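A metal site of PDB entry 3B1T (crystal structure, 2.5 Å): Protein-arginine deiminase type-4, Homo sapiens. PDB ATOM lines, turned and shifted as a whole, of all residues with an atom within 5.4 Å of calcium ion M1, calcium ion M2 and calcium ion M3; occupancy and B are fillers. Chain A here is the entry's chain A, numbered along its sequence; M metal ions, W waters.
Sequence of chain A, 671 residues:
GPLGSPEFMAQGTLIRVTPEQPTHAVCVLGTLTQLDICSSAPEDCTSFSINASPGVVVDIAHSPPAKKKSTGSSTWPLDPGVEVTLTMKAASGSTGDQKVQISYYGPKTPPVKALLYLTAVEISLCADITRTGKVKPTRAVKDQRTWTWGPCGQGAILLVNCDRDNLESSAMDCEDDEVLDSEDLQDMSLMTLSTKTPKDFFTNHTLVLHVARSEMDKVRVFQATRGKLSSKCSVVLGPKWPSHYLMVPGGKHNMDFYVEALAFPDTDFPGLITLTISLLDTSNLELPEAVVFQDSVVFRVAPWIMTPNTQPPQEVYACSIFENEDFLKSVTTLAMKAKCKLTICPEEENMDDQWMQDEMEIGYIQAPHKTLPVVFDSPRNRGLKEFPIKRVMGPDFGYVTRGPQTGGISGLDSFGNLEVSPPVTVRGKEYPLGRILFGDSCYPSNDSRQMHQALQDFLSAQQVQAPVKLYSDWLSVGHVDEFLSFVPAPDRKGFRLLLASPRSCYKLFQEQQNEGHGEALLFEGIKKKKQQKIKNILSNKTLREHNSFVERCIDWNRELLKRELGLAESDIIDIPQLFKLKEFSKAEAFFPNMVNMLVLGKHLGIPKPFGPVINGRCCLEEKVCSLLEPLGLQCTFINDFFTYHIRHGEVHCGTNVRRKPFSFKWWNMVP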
ATOM      1  N   ASN A 161      15.331 -22.754  20.995  1.00  0.00           N
ATOM      2  CA  ASN A 161      14.184 -22.628  21.866  1.00  0.00           C
ATOM      3  C   ASN A 161      13.984 -23.920  22.651  1.00  0.00           C
ATOM      4  O   ASN A 161      12.990 -24.643  22.526  1.00  0.00           O
ATOM      5  CB  ASN A 161      12.971 -22.247  21.017  1.00  0.00           C
ATOM      6  CG  ASN A 161      11.735 -21.901  21.837  1.00  0.00           C
ATOM      7  OD1 ASN A 161      11.794 -21.459  23.022  1.00  0.00           O
ATOM      8  ND2 ASN A 161      10.595 -22.100  21.212  1.00  0.00           N
ATOM      9  N   ASP A 163      14.036 -24.391  26.001  1.00  0.00           N
ATOM     10  CA  ASP A 163      13.448 -24.346  27.340  1.00  0.00           C
ATOM     11  C   ASP A 163      12.009 -24.886  27.288  1.00  0.00           C
ATOM     12  O   ASP A 163      11.563 -25.347  26.228  1.00  0.00           O
ATOM     13  CB  ASP A 163      13.517 -22.921  27.912  1.00  0.00           C
ATOM     14  CG  ASP A 163      12.454 -21.989  27.340  1.00  0.00           C
ATOM     15  OD1 ASP A 163      12.093 -22.137  26.146  1.00  0.00           O
ATOM     16  OD2 ASP A 163      11.974 -21.108  28.085  1.00  0.00           O
ATOM     17  N   ARG A 164      11.318 -24.840  28.433  1.00  0.00           N
ATOM     18  CA  ARG A 164       9.955 -25.379  28.561  1.00  0.00           C
ATOM     19  C   ARG A 164       8.997 -24.392  29.271  1.00  0.00           C
ATOM     20  O   ARG A 164       8.731 -24.524  30.472  1.00  0.00           O
ATOM     21  CB  ARG A 164       9.983 -26.732  29.296  1.00  0.00           C
ATOM     22  CG  ARG A 164       8.646 -27.475  29.307  1.00  0.00           C
ATOM     23  CD  ARG A 164       8.747 -28.850  29.958  1.00  0.00           C
ATOM     24  NE  ARG A 164       8.427 -28.812  31.403  1.00  0.00           N
ATOM     25  CZ  ARG A 164       9.231 -29.210  32.388  1.00  0.00           C
ATOM     26  NH1 ARG A 164      10.459 -29.703  32.155  1.00  0.00           N
ATOM     27  NH2 ARG A 164       8.807 -29.124  33.656  1.00  0.00           N
ATOM     28  N   ASP A 165       8.482 -23.434  28.502  1.00  0.00           N
ATOM     29  CA  ASP A 165       7.501 -22.457  28.991  1.00  0.00           C
ATOM     30  C   ASP A 165       6.077 -23.067  29.077  1.00  0.00           C
ATOM     31  O   ASP A 165       5.174 -22.450  29.659  1.00  0.00           O
ATOM     32  CB  ASP A 165       7.479 -21.196  28.103  1.00  0.00           C
ATOM     33  CG  ASP A 165       8.826 -20.461  28.052  1.00  0.00           C
ATOM     34  OD1 ASP A 165       9.342 -20.039  29.115  1.00  0.00           O
ATOM     35  OD2 ASP A 165       9.386 -20.282  26.940  1.00  0.00           O
ATOM     36  N   ASP A 173       9.988 -26.852  24.061  1.00  0.00           N
ATOM     37  CA  ASP A 173       9.083 -26.070  23.187  1.00  0.00           C
ATOM     38  C   ASP A 173       9.267 -26.368  21.667  1.00  0.00           C
ATOM     39  O   ASP A 173       8.277 -26.507  20.945  1.00  0.00           O
ATOM     40  CB  ASP A 173       9.262 -24.563  23.435  1.00  0.00           C
ATOM     41  CG  ASP A 173       8.845 -24.106  24.839  1.00  0.00           C
ATOM     42  OD1 ASP A 173       8.095 -24.830  25.546  1.00  0.00           O
ATOM     43  OD2 ASP A 173       9.266 -23.000  25.255  1.00  0.00           O
ATOM     44  N   CYS A 174      10.524 -26.454  21.203  1.00  0.00           N
ATOM     45  CA  CYS A 174      10.870 -26.609  19.766  1.00  0.00           C
ATOM     46  C   CYS A 174      10.698 -28.014  19.146  1.00  0.00           C
ATOM     47  O   CYS A 174      10.873 -28.199  17.935  1.00  0.00           O
ATOM     48  CB  CYS A 174      12.309 -26.109  19.501  1.00  0.00           C
ATOM     49  SG  CYS A 174      13.644 -27.029  20.339  1.00  0.00           S
ATOM     50  N   GLU A 175      10.325 -29.000  19.972  1.00  0.00           N
ATOM     51  CA  GLU A 175      10.048 -30.352  19.467  1.00  0.00           C
ATOM     52  C   GLU A 175       8.781 -30.435  18.596  1.00  0.00           C
ATOM     53  O   GLU A 175       8.565 -31.439  17.922  1.00  0.00           O
ATOM     54  CB  GLU A 175       9.972 -31.360  20.630  1.00  0.00           C
ATOM     55  CG  GLU A 175      11.306 -31.576  21.333  1.00  0.00           C
ATOM     56  CD  GLU A 175      11.380 -32.896  22.103  1.00  0.00           C
ATOM     57  OE1 GLU A 175      10.345 -33.584  22.217  1.00  0.00           O
ATOM     58  OE2 GLU A 175      12.478 -33.232  22.596  1.00  0.00           O
ATOM     59  N   ASP A 176       7.957 -29.387  18.625  1.00  0.00           N
ATOM     60  CA  ASP A 176       6.740 -29.335  17.803  1.00  0.00           C
ATOM     61  C   ASP A 176       6.632 -28.033  16.974  1.00  0.00           C
ATOM     62  O   ASP A 176       7.352 -27.058  17.224  1.00  0.00           O
ATOM     63  CB  ASP A 176       5.499 -29.534  18.678  1.00  0.00           C
ATOM     64  CG  ASP A 176       5.284 -28.398  19.672  1.00  0.00           C
ATOM     65  OD1 ASP A 176       4.662 -28.659  20.734  1.00  0.00           O
ATOM     66  OD2 ASP A 176       5.721 -27.256  19.425  1.00  0.00           O
ATOM     67  N   ASP A 177       5.699 -28.054  16.030  1.00  0.00           N
ATOM     68  CA  ASP A 177       5.505 -26.941  15.068  1.00  0.00           C
ATOM     69  C   ASP A 177       4.351 -26.010  15.484  1.00  0.00           C
ATOM     70  O   ASP A 177       3.568 -25.547  14.652  1.00  0.00           O
ATOM     71  CB  ASP A 177       5.308 -27.492  13.638  1.00  0.00           C
ATOM     72  CG  ASP A 177       4.420 -28.741  13.595  1.00  0.00           C
ATOM     73  OD1 ASP A 177       3.182 -28.606  13.687  1.00  0.00           O
ATOM     74  OD2 ASP A 177       4.958 -29.853  13.452  1.00  0.00           O
ATOM     75  N   GLU A 178       4.297 -25.704  16.786  1.00  0.00           N
ATOM     76  CA  GLU A 178       3.196 -24.942  17.381  1.00  0.00           C
ATOM     77  C   GLU A 178       3.711 -23.957  18.451  1.00  0.00           C
ATOM     78  O   GLU A 178       4.630 -24.270  19.219  1.00  0.00           O
ATOM     79  CB  GLU A 178       2.141 -25.891  17.996  1.00  0.00           C
ATOM     80  CG  GLU A 178       1.576 -26.968  17.026  1.00  0.00           C
ATOM     81  CD  GLU A 178       0.537 -27.890  17.675  1.00  0.00           C
ATOM     82  OE1 GLU A 178       0.337 -27.804  18.907  1.00  0.00           O
ATOM     83  OE2 GLU A 178      -0.079 -28.707  16.955  1.00  0.00           O
ATOM     84  N   VAL A 179       3.109 -22.759  18.484  1.00  0.00           N
ATOM     85  CA  VAL A 179       3.358 -21.775  19.534  1.00  0.00           C
ATOM     86  C   VAL A 179       2.135 -21.776  20.456  1.00  0.00           C
ATOM     87  O   VAL A 179       1.068 -21.280  20.078  1.00  0.00           O
ATOM     88  CB  VAL A 179       3.544 -20.338  18.975  1.00  0.00           C
ATOM     89  CG1 VAL A 179       3.913 -19.383  20.097  1.00  0.00           C
ATOM     90  CG2 VAL A 179       4.597 -20.318  17.912  1.00  0.00           C
ATOM     91  N   GLU A 183       4.018 -16.323  25.937  1.00  0.00           N
ATOM     92  CA  GLU A 183       5.293 -16.264  26.645  1.00  0.00           C
ATOM     93  C   GLU A 183       6.424 -16.851  25.794  1.00  0.00           C
ATOM     94  O   GLU A 183       7.563 -16.394  25.872  1.00  0.00           O
ATOM     95  CB  GLU A 183       5.217 -17.069  27.962  1.00  0.00           C
ATOM     96  CG  GLU A 183       4.291 -16.506  29.033  1.00  0.00           C
ATOM     97  CD  GLU A 183       2.853 -16.994  28.905  1.00  0.00           C
ATOM     98  OE1 GLU A 183       2.238 -17.294  29.948  1.00  0.00           O
ATOM     99  OE2 GLU A 183       2.331 -17.059  27.776  1.00  0.00           O
ATOM    100  N   ASP A 184       6.103 -17.870  25.012  1.00  0.00           N
ATOM    101  CA  ASP A 184       7.077 -18.540  24.191  1.00  0.00           C
ATOM    102  C   ASP A 184       7.613 -17.590  23.085  1.00  0.00           C
ATOM    103  O   ASP A 184       8.810 -17.683  22.722  1.00  0.00           O
ATOM    104  CB  ASP A 184       6.473 -19.839  23.606  1.00  0.00           C
ATOM    105  CG  ASP A 184       7.526 -20.738  22.939  1.00  0.00           C
ATOM    106  OD1 ASP A 184       7.192 -21.363  21.899  1.00  0.00           O
ATOM    107  OD2 ASP A 184       8.674 -20.827  23.432  1.00  0.00           O
ATOM    108  N   ASP A 187      11.038 -15.676  23.504  1.00  0.00           N
ATOM    109  CA  ASP A 187      12.313 -16.369  23.245  1.00  0.00           C
ATOM    110  C   ASP A 187      12.723 -16.286  21.782  1.00  0.00           C
ATOM    111  O   ASP A 187      13.839 -16.642  21.432  1.00  0.00           O
ATOM    112  CB  ASP A 187      12.223 -17.857  23.647  1.00  0.00           C
ATOM    113  CG  ASP A 187      12.106 -18.045  25.144  1.00  0.00           C
ATOM    114  OD1 ASP A 187      12.839 -17.372  25.892  1.00  0.00           O
ATOM    115  OD2 ASP A 187      11.282 -18.881  25.569  1.00  0.00           O
ATOM    116  N   ARG A 220      12.577 -22.829  12.784  1.00  0.00           N
ATOM    117  CA  ARG A 220      11.143 -22.772  12.565  1.00  0.00           C
ATOM    118  C   ARG A 220      10.658 -21.319  12.584  1.00  0.00           C
ATOM    119  O   ARG A 220      11.168 -20.496  13.365  1.00  0.00           O
ATOM    120  CB  ARG A 220      10.380 -23.610  13.587  1.00  0.00           C
ATOM    121  CG  ARG A 220       8.917 -23.777  13.184  1.00  0.00           C
ATOM    122  CD  ARG A 220       8.164 -24.614  14.116  1.00  0.00           C
ATOM    123  NE  ARG A 220       8.550 -26.016  14.029  1.00  0.00           N
ATOM    124  CZ  ARG A 220       9.238 -26.662  14.957  1.00  0.00           C
ATOM    125  NH1 ARG A 220       9.641 -26.049  16.060  1.00  0.00           N
ATOM    126  NH2 ARG A 220       9.533 -27.949  14.784  1.00  0.00           N
ATOM    127  N   PHE A 222       7.272 -18.687  12.421  1.00  0.00           N
ATOM    128  CA  PHE A 222       5.822 -18.512  12.543  1.00  0.00           C
ATOM    129  C   PHE A 222       5.387 -17.136  12.049  1.00  0.00           C
ATOM    130  O   PHE A 222       6.049 -16.137  12.343  1.00  0.00           O
ATOM    131  CB  PHE A 222       5.371 -18.652  14.004  1.00  0.00           C
ATOM    132  CG  PHE A 222       5.868 -19.880  14.691  1.00  0.00           C
ATOM    133  CD1 PHE A 222       7.110 -19.889  15.299  1.00  0.00           C
ATOM    134  CD2 PHE A 222       5.096 -21.027  14.767  1.00  0.00           C
ATOM    135  CE1 PHE A 222       7.576 -21.034  15.942  1.00  0.00           C
ATOM    136  CE2 PHE A 222       5.553 -22.166  15.427  1.00  0.00           C
ATOM    137  CZ  PHE A 222       6.785 -22.170  16.016  1.00  0.00           C
ATOM    138  N   GLU A 260      12.650 -19.218  15.668  1.00  0.00           N
ATOM    139  CA  GLU A 260      13.369 -20.002  16.694  1.00  0.00           C
ATOM    140  C   GLU A 260      14.309 -20.965  16.026  1.00  0.00           C
ATOM    141  O   GLU A 260      14.070 -21.361  14.909  1.00  0.00           O
ATOM    142  CB  GLU A 260      12.415 -20.834  17.556  1.00  0.00           C
ATOM    143  CG  GLU A 260      11.534 -21.774  16.706  1.00  0.00           C
ATOM    144  CD  GLU A 260      10.627 -22.636  17.497  1.00  0.00           C
ATOM    145  OE1 GLU A 260      10.404 -22.367  18.689  1.00  0.00           O
ATOM    146  OE2 GLU A 260      10.140 -23.621  16.923  1.00  0.00           O
ATOM    147  N   LYS A 370      16.761 -11.431  24.640  1.00  0.00           N
ATOM    148  CA  LYS A 370      16.486 -12.427  25.661  1.00  0.00           C
ATOM    149  C   LYS A 370      17.715 -13.252  26.094  1.00  0.00           C
ATOM    150  O   LYS A 370      18.415 -13.838  25.255  1.00  0.00           O
ATOM    151  CB  LYS A 370      15.390 -13.366  25.158  1.00  0.00           C
ATOM    152  CG  LYS A 370      15.065 -14.498  26.129  1.00  0.00           C
ATOM    153  CD  LYS A 370      14.669 -13.997  27.517  1.00  0.00           C
ATOM    154  CE  LYS A 370      13.221 -14.304  27.864  1.00  0.00           C
ATOM    155  NZ  LYS A 370      13.081 -14.432  29.363  1.00  0.00           N
ATOM    156  N   LEU A 372      18.737 -16.429  28.680  1.00  0.00           N
ATOM    157  CA  LEU A 372      18.182 -17.437  29.561  1.00  0.00           C
ATOM    158  C   LEU A 372      19.179 -18.481  29.914  1.00  0.00           C
ATOM    159  O   LEU A 372      20.067 -18.756  29.114  1.00  0.00           O
ATOM    160  CB  LEU A 372      16.931 -18.088  28.963  1.00  0.00           C
ATOM    161  CG  LEU A 372      16.940 -18.985  27.721  1.00  0.00           C
ATOM    162  CD1 LEU A 372      16.362 -20.377  28.040  1.00  0.00           C
ATOM    163  CD2 LEU A 372      16.141 -18.345  26.586  1.00  0.00           C
ATOM    164  N   PRO A 395      10.460 -23.165  32.804  1.00  0.00           N
ATOM    165  CA  PRO A 395      10.189 -21.797  32.373  1.00  0.00           C
ATOM    166  C   PRO A 395      11.413 -20.915  32.515  1.00  0.00           C
ATOM    167  O   PRO A 395      11.902 -20.682  33.628  1.00  0.00           O
ATOM    168  CB  PRO A 395       9.050 -21.341  33.289  1.00  0.00           C
ATOM    169  CG  PRO A 395       8.427 -22.595  33.795  1.00  0.00           C
ATOM    170  CD  PRO A 395       9.553 -23.575  33.898  1.00  0.00           C
ATOM    171  N   ASP A 396      11.895 -20.431  31.364  1.00  0.00           N
ATOM    172  CA  ASP A 396      13.176 -19.755  31.229  1.00  0.00           C
ATOM    173  C   ASP A 396      14.343 -20.586  31.785  1.00  0.00           C
ATOM    174  O   ASP A 396      15.203 -20.088  32.505  1.00  0.00           O
ATOM    175  CB  ASP A 396      13.114 -18.337  31.795  1.00  0.00           C
ATOM    176  CG  ASP A 396      12.327 -17.383  30.899  1.00  0.00           C
ATOM    177  OD1 ASP A 396      11.893 -17.795  29.782  1.00  0.00           O
ATOM    178  OD2 ASP A 396      12.139 -16.212  31.308  1.00  0.00           O
HETATM  179 CA    CA M   1      10.434 -20.985  24.957  1.00  0.00          CA
HETATM  180 CA    CA M   2      11.119 -18.929  27.924  1.00  0.00          CA
HETATM  181 CA    CA M   3       6.687 -25.143  19.931  1.00  0.00          CA
HETATM  182  O   HOH W   1       9.587 -16.852  27.554  1.00  0.00           O
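Calcium ion M3 is bound by O of Asp 173 (2.3 Å), O of Glu 178 (2.3 Å) and OD2 of Asp 176 (2.4 Å).
Calcium ion M2 is bound by OD1 of Asp 396 (2.3 Å), OD2 of Asp 163 (2.3 Å), OD2 of Asp 187 (2.4 Å), OD2 of Asp 165 (2.4 Å), OD1 of Asp 165 (2.4 Å) and water W1 (2.6 Å).
Calcium ion M2 has six donor atoms within binding distance.
Slightly farther from calcium ion M2 lies the side-chain carboxylate (OD1) of Asp 187 (3.1 Å).
Calcium ion M1 is bound by OD2 of Asp 184 (2.3 Å), OD1 of Asp 163 (2.3 Å), OD2 of Asp 173 (2.3 Å), OD2 of Asp 187 (2.3 Å), OD2 of Asp 165 (2.4 Å) and OD1 of Asn 161 (2.4 Å).
Calcium ion M1 has six donor atoms within binding distance.
The side-chain carboxylate of Glu 260 sits at hydrogen-bond distance from the side-chain amide nitrogen of Asn 161 (2.5 Å).
The side-chain carboxylate of Asp 396 lies within salt-bridge range of the side-chain amino group of Lys 370 (2.8 Å).
O of Asp 176 lies within hydrogen-bond range of NH1 of Arg 220 (2.8 Å).
The backbone carbonyl oxygen of Asn 161 sits at hydrogen-bond distance from the side-chain sulfur of Cys 174 (3.3 Å).
Within 4 Å of calcium ion M1: Asn 161, Asp 163, Asp 165, Asp 173, Asp 184 and Asp 187.
Within 4 Å of calcium ion M2: Asp 163, Asp 165, Asp 187 and Asp 396.
The nearest printed residue that does not touch calcium ion M2 is Glu 183 (4.8 Å).
Three residues have an atom within 4 Å of calcium ion M3: Asp 173, Asp 176 and Glu 178.
The nearest printed residue that does not touch calcium ion M3 is Cys 174 (4.2 Å).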
